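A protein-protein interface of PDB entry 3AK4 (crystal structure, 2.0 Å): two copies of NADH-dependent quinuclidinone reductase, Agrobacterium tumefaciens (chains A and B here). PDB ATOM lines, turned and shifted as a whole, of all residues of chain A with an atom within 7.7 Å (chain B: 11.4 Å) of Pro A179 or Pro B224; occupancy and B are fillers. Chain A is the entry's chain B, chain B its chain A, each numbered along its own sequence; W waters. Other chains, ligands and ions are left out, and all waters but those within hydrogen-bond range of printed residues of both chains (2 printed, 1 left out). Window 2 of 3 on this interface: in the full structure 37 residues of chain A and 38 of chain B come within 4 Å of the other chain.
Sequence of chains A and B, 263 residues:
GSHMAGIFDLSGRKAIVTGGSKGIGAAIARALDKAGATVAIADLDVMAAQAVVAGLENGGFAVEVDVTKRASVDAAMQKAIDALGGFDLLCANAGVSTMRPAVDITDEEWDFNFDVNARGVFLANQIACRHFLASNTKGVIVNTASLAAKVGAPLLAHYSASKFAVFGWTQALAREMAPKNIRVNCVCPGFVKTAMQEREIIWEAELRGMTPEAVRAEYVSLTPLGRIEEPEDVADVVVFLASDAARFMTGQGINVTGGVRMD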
ATOM      1  N   LEU A 133       8.312 -25.629  21.750  1.00  0.00           N
ATOM      2  CA  LEU A 133       7.122 -25.314  22.551  1.00  0.00           C
ATOM      3  C   LEU A 133       7.400 -25.353  24.059  1.00  0.00           C
ATOM      4  O   LEU A 133       6.871 -24.509  24.811  1.00  0.00           O
ATOM      5  CB  LEU A 133       5.916 -26.193  22.178  1.00  0.00           C
ATOM      6  CG  LEU A 133       5.248 -25.890  20.827  1.00  0.00           C
ATOM      7  CD1 LEU A 133       4.397 -27.096  20.405  1.00  0.00           C
ATOM      8  CD2 LEU A 133       4.419 -24.577  20.844  1.00  0.00           C
ATOM      9  N   LEU A 173       2.068 -28.753   8.867  1.00  0.00           N
ATOM     10  CA  LEU A 173       2.791 -28.384  10.102  1.00  0.00           C
ATOM     11  C   LEU A 173       2.887 -26.848  10.226  1.00  0.00           C
ATOM     12  O   LEU A 173       2.672 -26.285  11.317  1.00  0.00           O
ATOM     13  CB  LEU A 173       4.195 -29.043  10.191  1.00  0.00           C
ATOM     14  CG  LEU A 173       4.967 -28.754  11.494  1.00  0.00           C
ATOM     15  CD1 LEU A 173       4.212 -29.277  12.749  1.00  0.00           C
ATOM     16  CD2 LEU A 173       6.404 -29.265  11.446  1.00  0.00           C
ATOM     17  N   ALA A 174       3.186 -26.177   9.111  1.00  0.00           N
ATOM     18  CA  ALA A 174       3.226 -24.713   9.093  1.00  0.00           C
ATOM     19  C   ALA A 174       1.922 -24.123   9.599  1.00  0.00           C
ATOM     20  O   ALA A 174       1.922 -23.177  10.411  1.00  0.00           O
ATOM     21  CB  ALA A 174       3.549 -24.176   7.672  1.00  0.00           C
ATOM     22  N   ARG A 175       0.793 -24.663   9.128  1.00  0.00           N
ATOM     23  CA  ARG A 175      -0.511 -24.158   9.571  1.00  0.00           C
ATOM     24  C   ARG A 175      -0.730 -24.341  11.097  1.00  0.00           C
ATOM     25  O   ARG A 175      -1.246 -23.437  11.759  1.00  0.00           O
ATOM     26  CB  ARG A 175      -1.684 -24.694   8.696  1.00  0.00           C
ATOM     27  CG  ARG A 175      -1.660 -24.105   7.261  1.00  0.00           C
ATOM     28  CD  ARG A 175      -2.886 -24.450   6.355  1.00  0.00           C
ATOM     29  NE  ARG A 175      -2.732 -23.906   4.964  1.00  0.00           N
ATOM     30  CZ  ARG A 175      -2.995 -22.644   4.564  1.00  0.00           C
ATOM     31  NH1 ARG A 175      -3.426 -21.717   5.415  1.00  0.00           N
ATOM     32  NH2 ARG A 175      -2.806 -22.290   3.285  1.00  0.00           N
ATOM     33  N   GLU A 176      -0.274 -25.469  11.660  1.00  0.00           N
ATOM     34  CA  GLU A 176      -0.412 -25.700  13.107  1.00  0.00           C
ATOM     35  C   GLU A 176       0.542 -24.856  13.937  1.00  0.00           C
ATOM     36  O   GLU A 176       0.197 -24.449  15.075  1.00  0.00           O
ATOM     37  CB  GLU A 176      -0.236 -27.188  13.475  1.00  0.00           C
ATOM     38  CG  GLU A 176      -1.248 -28.099  12.765  1.00  0.00           C
ATOM     39  CD  GLU A 176      -1.306 -29.504  13.334  1.00  0.00           C
ATOM     40  OE1 GLU A 176      -1.156 -29.666  14.572  1.00  0.00           O
ATOM     41  OE2 GLU A 176      -1.504 -30.448  12.540  1.00  0.00           O
ATOM     42  N   MET A 177       1.731 -24.587  13.387  1.00  0.00           N
ATOM     43  CA  MET A 177       2.817 -23.956  14.150  1.00  0.00           C
ATOM     44  C   MET A 177       2.756 -22.423  14.110  1.00  0.00           C
ATOM     45  O   MET A 177       3.245 -21.746  15.028  1.00  0.00           O
ATOM     46  CB  MET A 177       4.206 -24.479  13.681  1.00  0.00           C
ATOM     47  CG  MET A 177       4.518 -25.926  14.153  1.00  0.00           C
ATOM     48  SD  MET A 177       4.486 -26.087  15.969  1.00  0.00           S
ATOM     49  CE  MET A 177       2.906 -26.903  16.217  1.00  0.00           C
ATOM     50  N   ALA A 178       2.163 -21.876  13.052  1.00  0.00           N
ATOM     51  CA  ALA A 178       2.076 -20.405  12.887  1.00  0.00           C
ATOM     52  C   ALA A 178       1.471 -19.615  14.064  1.00  0.00           C
ATOM     53  O   ALA A 178       2.002 -18.554  14.424  1.00  0.00           O
ATOM     54  CB  ALA A 178       1.375 -20.052  11.562  1.00  0.00           C
ATOM     55  N   PRO A 179       0.344 -20.104  14.654  1.00  0.00           N
ATOM     56  CA  PRO A 179      -0.170 -19.431  15.853  1.00  0.00           C
ATOM     57  C   PRO A 179       0.766 -19.491  17.057  1.00  0.00           C
ATOM     58  O   PRO A 179       0.587 -18.705  17.985  1.00  0.00           O
ATOM     59  CB  PRO A 179      -1.481 -20.185  16.158  1.00  0.00           C
ATOM     60  CG  PRO A 179      -1.810 -20.917  14.918  1.00  0.00           C
ATOM     61  CD  PRO A 179      -0.528 -21.227  14.255  1.00  0.00           C
ATOM     62  N   LYS A 180       1.736 -20.410  17.057  1.00  0.00           N
ATOM     63  CA  LYS A 180       2.743 -20.484  18.120  1.00  0.00           C
ATOM     64  C   LYS A 180       4.028 -19.708  17.738  1.00  0.00           C
ATOM     65  O   LYS A 180       5.033 -19.759  18.471  1.00  0.00           O
ATOM     66  CB  LYS A 180       3.075 -21.950  18.455  1.00  0.00           C
ATOM     67  CG  LYS A 180       1.852 -22.885  18.611  1.00  0.00           C
ATOM     68  CD  LYS A 180       1.156 -22.753  19.953  1.00  0.00           C
ATOM     69  CE  LYS A 180      -0.061 -23.745  20.041  1.00  0.00           C
ATOM     70  NZ  LYS A 180      -1.235 -23.208  20.853  1.00  0.00           N
ATOM     71  N   ASN A 181       3.992 -19.011  16.591  1.00  0.00           N
ATOM     72  CA  ASN A 181       5.136 -18.203  16.106  1.00  0.00           C
ATOM     73  C   ASN A 181       6.388 -19.029  15.735  1.00  0.00           C
ATOM     74  O   ASN A 181       7.539 -18.599  15.906  1.00  0.00           O
ATOM     75  CB  ASN A 181       5.441 -17.060  17.109  1.00  0.00           C
ATOM     76  CG  ASN A 181       4.357 -15.967  17.097  1.00  0.00           C
ATOM     77  OD1 ASN A 181       4.048 -15.395  16.042  1.00  0.00           O
ATOM     78  ND2 ASN A 181       3.782 -15.674  18.266  1.00  0.00           N
ATOM     79  N   ILE A 182       6.117 -20.228  15.225  1.00  0.00           N
ATOM     80  CA  ILE A 182       7.110 -21.135  14.706  1.00  0.00           C
ATOM     81  C   ILE A 182       6.885 -21.202  13.191  1.00  0.00           C
ATOM     82  O   ILE A 182       5.753 -21.448  12.743  1.00  0.00           O
ATOM     83  CB  ILE A 182       7.028 -22.551  15.397  1.00  0.00           C
ATOM     84  CG1 ILE A 182       7.538 -22.464  16.847  1.00  0.00           C
ATOM     85  CG2 ILE A 182       7.854 -23.625  14.641  1.00  0.00           C
ATOM     86  CD1 ILE A 182       7.017 -23.604  17.749  1.00  0.00           C
ATOM     87  N   PHE A 248       7.797 -13.184   7.658  1.00  0.00           N
ATOM     88  CA  PHE A 248       6.375 -13.285   7.264  1.00  0.00           C
ATOM     89  C   PHE A 248       6.150 -14.379   6.179  1.00  0.00           C
ATOM     90  O   PHE A 248       5.241 -14.278   5.338  1.00  0.00           O
ATOM     91  CB  PHE A 248       5.797 -11.905   6.848  1.00  0.00           C
ATOM     92  CG  PHE A 248       4.351 -11.693   7.260  1.00  0.00           C
ATOM     93  CD1 PHE A 248       3.995 -11.644   8.611  1.00  0.00           C
ATOM     94  CD2 PHE A 248       3.350 -11.566   6.312  1.00  0.00           C
ATOM     95  CE1 PHE A 248       2.660 -11.451   8.999  1.00  0.00           C
ATOM     96  CE2 PHE A 248       1.998 -11.379   6.712  1.00  0.00           C
ATOM     97  CZ  PHE A 248       1.670 -11.333   8.053  1.00  0.00           C
ATOM     98  N   THR A 250       5.840 -18.662   5.665  1.00  0.00           N
ATOM     99  CA  THR A 250       5.752 -20.020   6.228  1.00  0.00           C
ATOM    100  C   THR A 250       4.918 -20.983   5.368  1.00  0.00           C
ATOM    101  O   THR A 250       3.991 -20.549   4.677  1.00  0.00           O
ATOM    102  CB  THR A 250       5.269 -20.001   7.722  1.00  0.00           C
ATOM    103  OG1 THR A 250       5.562 -21.265   8.311  1.00  0.00           O
ATOM    104  CG2 THR A 250       3.730 -19.648   7.864  1.00  0.00           C
ATOM    105  N   LEU B 147      -0.901 -11.544  -3.761  1.00  0.00           N
ATOM    106  CA  LEU B 147      -1.716 -12.741  -3.447  1.00  0.00           C
ATOM    107  C   LEU B 147      -2.767 -13.020  -4.540  1.00  0.00           C
ATOM    108  O   LEU B 147      -2.982 -14.184  -4.918  1.00  0.00           O
ATOM    109  CB  LEU B 147      -2.411 -12.600  -2.082  1.00  0.00           C
ATOM    110  CG  LEU B 147      -3.433 -13.680  -1.628  1.00  0.00           C
ATOM    111  CD1 LEU B 147      -2.770 -15.034  -1.546  1.00  0.00           C
ATOM    112  CD2 LEU B 147      -4.082 -13.316  -0.293  1.00  0.00           C
ATOM    113  N   GLY B 190       0.566 -10.273   0.972  1.00  0.00           N
ATOM    114  CA  GLY B 190      -0.771 -10.544   1.509  1.00  0.00           C
ATOM    115  C   GLY B 190      -1.540  -9.278   1.864  1.00  0.00           C
ATOM    116  O   GLY B 190      -1.710  -8.395   1.022  1.00  0.00           O
ATOM    117  N   PHE B 191      -2.007  -9.186   3.111  1.00  0.00           N
ATOM    118  CA  PHE B 191      -2.842  -8.051   3.515  1.00  0.00           C
ATOM    119  C   PHE B 191      -1.968  -6.971   4.175  1.00  0.00           C
ATOM    120  O   PHE B 191      -1.868  -6.889   5.415  1.00  0.00           O
ATOM    121  CB  PHE B 191      -3.988  -8.523   4.450  1.00  0.00           C
ATOM    122  CG  PHE B 191      -4.789  -9.713   3.922  1.00  0.00           C
ATOM    123  CD1 PHE B 191      -5.569  -9.611   2.751  1.00  0.00           C
ATOM    124  CD2 PHE B 191      -4.781 -10.937   4.611  1.00  0.00           C
ATOM    125  CE1 PHE B 191      -6.297 -10.748   2.260  1.00  0.00           C
ATOM    126  CE2 PHE B 191      -5.501 -12.047   4.138  1.00  0.00           C
ATOM    127  CZ  PHE B 191      -6.284 -11.943   2.969  1.00  0.00           C
ATOM    128  N   ARG B 216     -11.013  -5.754   8.558  1.00  0.00           N
ATOM    129  CA  ARG B 216      -9.590  -5.884   8.941  1.00  0.00           C
ATOM    130  C   ARG B 216      -9.336  -7.064   9.895  1.00  0.00           C
ATOM    131  O   ARG B 216      -8.325  -7.782   9.762  1.00  0.00           O
ATOM    132  CB  ARG B 216      -9.034  -4.586   9.547  1.00  0.00           C
ATOM    133  CG  ARG B 216      -7.524  -4.442   9.328  1.00  0.00           C
ATOM    134  CD  ARG B 216      -6.838  -3.458  10.254  1.00  0.00           C
ATOM    135  NE  ARG B 216      -7.452  -2.121  10.268  1.00  0.00           N
ATOM    136  CZ  ARG B 216      -7.038  -1.060   9.570  1.00  0.00           C
ATOM    137  NH1 ARG B 216      -5.991  -1.123   8.739  1.00  0.00           N
ATOM    138  NH2 ARG B 216      -7.673   0.094   9.716  1.00  0.00           N
ATOM    139  N   ALA B 217     -10.251  -7.258  10.846  1.00  0.00           N
ATOM    140  CA  ALA B 217     -10.178  -8.385  11.776  1.00  0.00           C
ATOM    141  C   ALA B 217     -10.231  -9.732  11.051  1.00  0.00           C
ATOM    142  O   ALA B 217      -9.535 -10.677  11.425  1.00  0.00           O
ATOM    143  CB  ALA B 217     -11.266  -8.300  12.810  1.00  0.00           C
ATOM    144  N   GLU B 218     -11.056  -9.797  10.010  1.00  0.00           N
ATOM    145  CA  GLU B 218     -11.182 -10.986   9.189  1.00  0.00           C
ATOM    146  C   GLU B 218      -9.885 -11.326   8.419  1.00  0.00           C
ATOM    147  O   GLU B 218      -9.479 -12.490   8.413  1.00  0.00           O
ATOM    148  CB  GLU B 218     -12.387 -10.842   8.260  1.00  0.00           C
ATOM    149  CG  GLU B 218     -12.622 -12.052   7.338  1.00  0.00           C
ATOM    150  CD  GLU B 218     -13.820 -11.834   6.414  1.00  0.00           C
ATOM    151  OE1 GLU B 218     -14.963 -11.650   6.945  1.00  0.00           O
ATOM    152  OE2 GLU B 218     -13.605 -11.835   5.166  1.00  0.00           O
ATOM    153  N   TYR B 219      -9.237 -10.327   7.802  1.00  0.00           N
ATOM    154  CA  TYR B 219      -7.884 -10.473   7.242  1.00  0.00           C
ATOM    155  C   TYR B 219      -6.921 -11.111   8.263  1.00  0.00           C
ATOM    156  O   TYR B 219      -6.246 -12.086   7.950  1.00  0.00           O
ATOM    157  CB  TYR B 219      -7.282  -9.128   6.789  1.00  0.00           C
ATOM    158  CG  TYR B 219      -7.992  -8.348   5.685  1.00  0.00           C
ATOM    159  CD1 TYR B 219      -8.972  -8.922   4.864  1.00  0.00           C
ATOM    160  CD2 TYR B 219      -7.656  -7.015   5.462  1.00  0.00           C
ATOM    161  CE1 TYR B 219      -9.615  -8.156   3.859  1.00  0.00           C
ATOM    162  CE2 TYR B 219      -8.251  -6.264   4.463  1.00  0.00           C
ATOM    163  CZ  TYR B 219      -9.231  -6.830   3.666  1.00  0.00           C
ATOM    164  OH  TYR B 219      -9.801  -6.025   2.678  1.00  0.00           O
ATOM    165  N   VAL B 220      -6.896 -10.571   9.486  1.00  0.00           N
ATOM    166  CA  VAL B 220      -6.054 -11.129  10.541  1.00  0.00           C
ATOM    167  C   VAL B 220      -6.382 -12.618  10.842  1.00  0.00           C
ATOM    168  O   VAL B 220      -5.471 -13.448  10.939  1.00  0.00           O
ATOM    169  CB  VAL B 220      -6.040 -10.264  11.839  1.00  0.00           C
ATOM    170  CG1 VAL B 220      -5.177 -10.949  12.923  1.00  0.00           C
ATOM    171  CG2 VAL B 220      -5.465  -8.846  11.542  1.00  0.00           C
ATOM    172  N   SER B 221      -7.670 -12.939  10.956  1.00  0.00           N
ATOM    173  CA  SER B 221      -8.102 -14.301  11.308  1.00  0.00           C
ATOM    174  C   SER B 221      -7.793 -15.330  10.190  1.00  0.00           C
ATOM    175  O   SER B 221      -7.542 -16.539  10.455  1.00  0.00           O
ATOM    176  CB  SER B 221      -9.589 -14.309  11.734  1.00  0.00           C
ATOM    177  OG  SER B 221     -10.425 -14.414  10.587  1.00  0.00           O
ATOM    178  N   LEU B 222      -7.752 -14.824   8.956  1.00  0.00           N
ATOM    179  CA  LEU B 222      -7.321 -15.598   7.784  1.00  0.00           C
ATOM    180  C   LEU B 222      -5.789 -15.797   7.650  1.00  0.00           C
ATOM    181  O   LEU B 222      -5.339 -16.543   6.764  1.00  0.00           O
ATOM    182  CB  LEU B 222      -7.866 -14.964   6.488  1.00  0.00           C
ATOM    183  CG  LEU B 222      -9.390 -15.004   6.288  1.00  0.00           C
ATOM    184  CD1 LEU B 222      -9.796 -14.146   5.086  1.00  0.00           C
ATOM    185  CD2 LEU B 222      -9.924 -16.412   6.124  1.00  0.00           C
ATOM    186  N   THR B 223      -5.020 -15.146   8.522  1.00  0.00           N
ATOM    187  CA  THR B 223      -3.539 -15.152   8.451  1.00  0.00           C
ATOM    188  C   THR B 223      -2.960 -16.058   9.532  1.00  0.00           C
ATOM    189  O   THR B 223      -3.048 -15.721  10.719  1.00  0.00           O
ATOM    190  CB  THR B 223      -2.966 -13.719   8.615  1.00  0.00           C
ATOM    191  OG1 THR B 223      -3.588 -12.853   7.654  1.00  0.00           O
ATOM    192  CG2 THR B 223      -1.402 -13.681   8.450  1.00  0.00           C
ATOM    193  N   PRO B 224      -2.403 -17.229   9.141  1.00  0.00           N
ATOM    194  CA  PRO B 224      -1.815 -18.144  10.169  1.00  0.00           C
ATOM    195  C   PRO B 224      -0.813 -17.505  11.153  1.00  0.00           C
ATOM    196  O   PRO B 224      -0.828 -17.816  12.359  1.00  0.00           O
ATOM    197  CB  PRO B 224      -1.169 -19.260   9.325  1.00  0.00           C
ATOM    198  CG  PRO B 224      -2.043 -19.283   8.023  1.00  0.00           C
ATOM    199  CD  PRO B 224      -2.380 -17.818   7.780  1.00  0.00           C
ATOM    200  N   LEU B 225       0.046 -16.611  10.662  1.00  0.00           N
ATOM    201  CA  LEU B 225       0.976 -15.959  11.576  1.00  0.00           C
ATOM    202  C   LEU B 225       0.309 -14.898  12.492  1.00  0.00           C
ATOM    203  O   LEU B 225       0.972 -14.340  13.364  1.00  0.00           O
ATOM    204  CB  LEU B 225       2.197 -15.400  10.825  1.00  0.00           C
ATOM    205  CG  LEU B 225       3.253 -16.406  10.381  1.00  0.00           C
ATOM    206  CD1 LEU B 225       4.286 -15.710   9.506  1.00  0.00           C
ATOM    207  CD2 LEU B 225       3.917 -17.056  11.643  1.00  0.00           C
ATOM    208  N   GLY B 226      -0.989 -14.631  12.291  1.00  0.00           N
ATOM    209  CA  GLY B 226      -1.807 -13.921  13.285  1.00  0.00           C
ATOM    210  C   GLY B 226      -1.693 -12.397  13.429  1.00  0.00           C
ATOM    211  O   GLY B 226      -2.079 -11.833  14.465  1.00  0.00           O
ATOM    212  N   ARG B 227      -1.196 -11.711  12.407  1.00  0.00           N
ATOM    213  CA  ARG B 227      -1.129 -10.248  12.490  1.00  0.00           C
ATOM    214  C   ARG B 227      -1.281  -9.677  11.092  1.00  0.00           C
ATOM    215  O   ARG B 227      -1.057 -10.384  10.101  1.00  0.00           O
ATOM    216  CB  ARG B 227       0.189  -9.764  13.150  1.00  0.00           C
ATOM    217  CG  ARG B 227       1.477 -10.164  12.385  1.00  0.00           C
ATOM    218  CD  ARG B 227       2.703  -9.370  12.882  1.00  0.00           C
ATOM    219  NE  ARG B 227       4.003  -9.756  12.275  1.00  0.00           N
ATOM    220  CZ  ARG B 227       4.538  -9.205  11.172  1.00  0.00           C
ATOM    221  NH1 ARG B 227       3.881  -8.248  10.474  1.00  0.00           N
ATOM    222  NH2 ARG B 227       5.746  -9.612  10.745  1.00  0.00           N
ATOM    223  N   ILE B 228      -1.657  -8.403  11.023  1.00  0.00           N
ATOM    224  CA  ILE B 228      -1.653  -7.672   9.749  1.00  0.00           C
ATOM    225  C   ILE B 228      -0.209  -7.543   9.222  1.00  0.00           C
ATOM    226  O   ILE B 228       0.753  -7.467   9.992  1.00  0.00           O
ATOM    227  CB  ILE B 228      -2.425  -6.293   9.869  1.00  0.00           C
ATOM    228  CG1 ILE B 228      -3.120  -5.916   8.552  1.00  0.00           C
ATOM    229  CG2 ILE B 228      -1.518  -5.180  10.345  1.00  0.00           C
ATOM    230  CD1 ILE B 228      -4.216  -6.895   8.105  1.00  0.00           C
ATOM    231  N   GLU B 229      -0.057  -7.547   7.908  1.00  0.00           N
ATOM    232  CA  GLU B 229       1.258  -7.430   7.300  1.00  0.00           C
ATOM    233  C   GLU B 229       1.760  -5.970   7.251  1.00  0.00           C
ATOM    234  O   GLU B 229       0.960  -5.037   7.111  1.00  0.00           O
ATOM    235  CB  GLU B 229       1.241  -8.041   5.902  1.00  0.00           C
ATOM    236  CG  GLU B 229       2.644  -8.233   5.299  1.00  0.00           C
ATOM    237  CD  GLU B 229       2.649  -9.064   4.009  1.00  0.00           C
ATOM    238  OE1 GLU B 229       1.569  -9.431   3.493  1.00  0.00           O
ATOM    239  OE2 GLU B 229       3.745  -9.337   3.506  1.00  0.00           O
ATOM    240  N   ASN B 255       5.633 -15.978  -2.388  1.00  0.00           N
ATOM    241  CA  ASN B 255       4.535 -15.575  -1.534  1.00  0.00           C
ATOM    242  C   ASN B 255       5.078 -14.934  -0.266  1.00  0.00           C
ATOM    243  O   ASN B 255       5.990 -15.480   0.367  1.00  0.00           O
ATOM    244  CB  ASN B 255       3.646 -16.785  -1.174  1.00  0.00           C
ATOM    245  CG  ASN B 255       2.933 -17.386  -2.377  1.00  0.00           C
ATOM    246  OD1 ASN B 255       2.500 -16.678  -3.299  1.00  0.00           O
ATOM    247  ND2 ASN B 255       2.816 -18.718  -2.378  1.00  0.00           N
ATOM    248  N   VAL B 256       4.530 -13.775   0.100  1.00  0.00           N
ATOM    249  CA  VAL B 256       4.887 -13.147   1.381  1.00  0.00           C
ATOM    250  C   VAL B 256       3.576 -12.715   2.061  1.00  0.00           C
ATOM    251  O   VAL B 256       3.174 -11.543   1.996  1.00  0.00           O
ATOM    252  CB  VAL B 256       5.945 -11.951   1.266  1.00  0.00           C
ATOM    253  CG1 VAL B 256       6.435 -11.524   2.677  1.00  0.00           C
ATOM    254  CG2 VAL B 256       7.185 -12.329   0.384  1.00  0.00           C
ATOM    255  N   THR B 257       2.910 -13.680   2.693  1.00  0.00           N
ATOM    256  CA  THR B 257       1.494 -13.541   3.131  1.00  0.00           C
ATOM    257  C   THR B 257       1.260 -14.012   4.575  1.00  0.00           C
ATOM    258  O   THR B 257       0.134 -13.938   5.087  1.00  0.00           O
ATOM    259  CB  THR B 257       0.504 -14.345   2.178  1.00  0.00           C
ATOM    260  OG1 THR B 257       0.723 -15.748   2.342  1.00  0.00           O
ATOM    261  CG2 THR B 257       0.771 -14.014   0.705  1.00  0.00           C
ATOM    262  N   GLY B 258       2.317 -14.483   5.233  1.00  0.00           N
ATOM    263  CA  GLY B 258       2.177 -14.960   6.611  1.00  0.00           C
ATOM    264  C   GLY B 258       1.432 -16.287   6.683  1.00  0.00           C
ATOM    265  O   GLY B 258       0.744 -16.547   7.673  1.00  0.00           O
ATOM    266  N   GLY B 259       1.583 -17.104   5.635  1.00  0.00           N
ATOM    267  CA  GLY B 259       0.979 -18.454   5.518  1.00  0.00           C
ATOM    268  C   GLY B 259      -0.398 -18.569   4.842  1.00  0.00           C
ATOM    269  O   GLY B 259      -0.974 -19.664   4.788  1.00  0.00           O
ATOM    270  N   VAL B 260      -0.911 -17.470   4.303  1.00  0.00           N
ATOM    271  CA  VAL B 260      -2.261 -17.452   3.660  1.00  0.00           C
ATOM    272  C   VAL B 260      -2.272 -18.289   2.382  1.00  0.00           C
ATOM    273  O   VAL B 260      -3.198 -19.086   2.138  1.00  0.00           O
ATOM    274  CB  VAL B 260      -2.762 -15.993   3.364  1.00  0.00           C
ATOM    275  CG1 VAL B 260      -4.090 -15.998   2.508  1.00  0.00           C
ATOM    276  CG2 VAL B 260      -2.959 -15.226   4.639  1.00  0.00           C
ATOM    277  N   ARG B 261      -1.201 -18.138   1.604  1.00  0.00           N
ATOM    278  CA  ARG B 261      -0.983 -18.926   0.392  1.00  0.00           C
ATOM    279  C   ARG B 261       0.358 -19.682   0.435  1.00  0.00           C
ATOM    280  O   ARG B 261       1.403 -19.090   0.743  1.00  0.00           O
ATOM    281  CB  ARG B 261      -1.024 -17.975  -0.821  1.00  0.00           C
ATOM    282  CG  ARG B 261      -0.755 -18.604  -2.183  1.00  0.00           C
ATOM    283  CD  ARG B 261      -1.736 -19.760  -2.529  1.00  0.00           C
ATOM    284  NE  ARG B 261      -1.427 -20.319  -3.847  1.00  0.00           N
ATOM    285  CZ  ARG B 261      -2.289 -20.948  -4.649  1.00  0.00           C
ATOM    286  NH1 ARG B 261      -3.542 -21.160  -4.261  1.00  0.00           N
ATOM    287  NH2 ARG B 261      -1.865 -21.396  -5.837  1.00  0.00           N
ATOM    288  N   MET B 262       0.331 -20.981   0.113  1.00  0.00           N
ATOM    289  CA  MET B 262       1.549 -21.817   0.069  1.00  0.00           C
ATOM    290  C   MET B 262       1.765 -22.461  -1.310  1.00  0.00           C
ATOM    291  O   MET B 262       0.916 -23.234  -1.782  1.00  0.00           O
ATOM    292  CB  MET B 262       1.481 -22.932   1.130  1.00  0.00           C
ATOM    293  CG  MET B 262       1.377 -22.420   2.577  1.00  0.00           C
ATOM    294  SD  MET B 262       0.840 -23.587   3.840  1.00  0.00           S
ATOM    295  CE  MET B 262       0.987 -22.453   5.211  1.00  0.00           C
HETATM  296  O   HOH W   1      -2.173 -22.414   0.190  1.00  0.00           O
HETATM  297  O   HOH W   2      -5.195 -19.720   3.827  1.00  0.00           O
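The backbone carbonyl oxygen (O) of Val B260 lies within hydrogen-bond range of the guanidinium group (NH2) of Arg A175 (3.4 Å). The side-chain sulfur (SD) of Met B262 sits at hydrogen-bond distance from the guanidinium group (NE) of Arg A175. The backbone carbonyl oxygen of Phe A248 lies within hydrogen-bond range of the backbone NH of Gly B258 (2.9 Å). N of Pro A179 lies close to O of Pro B224 (3.4 Å). The backbone carbonyl oxygen (O) of Gly B259 sits at hydrogen-bond distance from the guanidinium group (NH1) of Arg A175, at 3.3 Å.
Water W2 lies within hydrogen-bond range of the backbone carbonyl oxygen of Val B260 and the guanidinium group of Arg A175. Water W1 bridges the backbone NH of Met B262 (2.9 Å) and the guanidinium group of Arg A175 (3.2 Å).
The backbone NH (N) of Leu B225 is in hydrogen-bond range of the backbone carbonyl oxygen (O) of Gly B258 (3.1 Å). O of Phe B191 sits at hydrogen-bond distance from N of Glu B229 (3.2 Å). The side-chain hydroxyl (OG1) of Thr B257 sits at hydrogen-bond distance from the backbone NH (N) of Val B260 (3.1 Å). The side-chain carboxylate (OE2) of Glu B229 lies close to the backbone carbonyl oxygen (O) of Val B256, 2.7 Å away. N of Gly B190 sits at hydrogen-bond distance from OE1 of Glu B229. The backbone NH of Gly B190 sits at hydrogen-bond distance from the backbone carbonyl oxygen of Val B256 (3.1 Å).
Leu A133 touches none of the printed residues of chain B. No residue of chain B comes within 4 Å of Met A177. Of chain B, only Pro B224 and Leu B225 come within 4 Å of Ala A178. Pro A179 touches one residue of chain B. No residue of chain B comes within 4 Å of Lys A180. Ile A182 touches none of the printed residues of chain B. Of the printed residues of chain B, Thr A250 touches Gly B259 and Met B262. Pro B224 touches three residues of chain A. Of the printed residues of chain A, Val B260 touches Arg A175. The nearest printed residue of chain A that does not touch Arg B227 is Asn A181 (6.8 Å).
No position is printed for both chains.
Among the printed residues, pairs that only touch across the chains: Ala A178 with Pro B224, Phe A248 with Arg B227, Phe A248 with Thr B257, Phe A248 with Glu B229, Thr A250 with Met B262, Ala A178 with Leu B225, Thr A250 with Gly B259, Arg A175 with Pro B224, Phe A248 with Thr B223, Phe A248 with Leu B225, Ala A174 with Met B262 and Phe A248 with Val B256.
Hydrophobic or aromatic side chains of chain B that line the printed part of chain A: Pro B224, Leu B225 and Met B262. Hydrophobic or aromatic side chains of chain A within 4 Å of the printed part of chain B: Ala A174, Ala A178, Pro A179 and Phe A248. Among the printed residues, no Asp or Glu carboxylate lies within 4 Å of a Lys or Arg side-chain nitrogen of the other chain.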
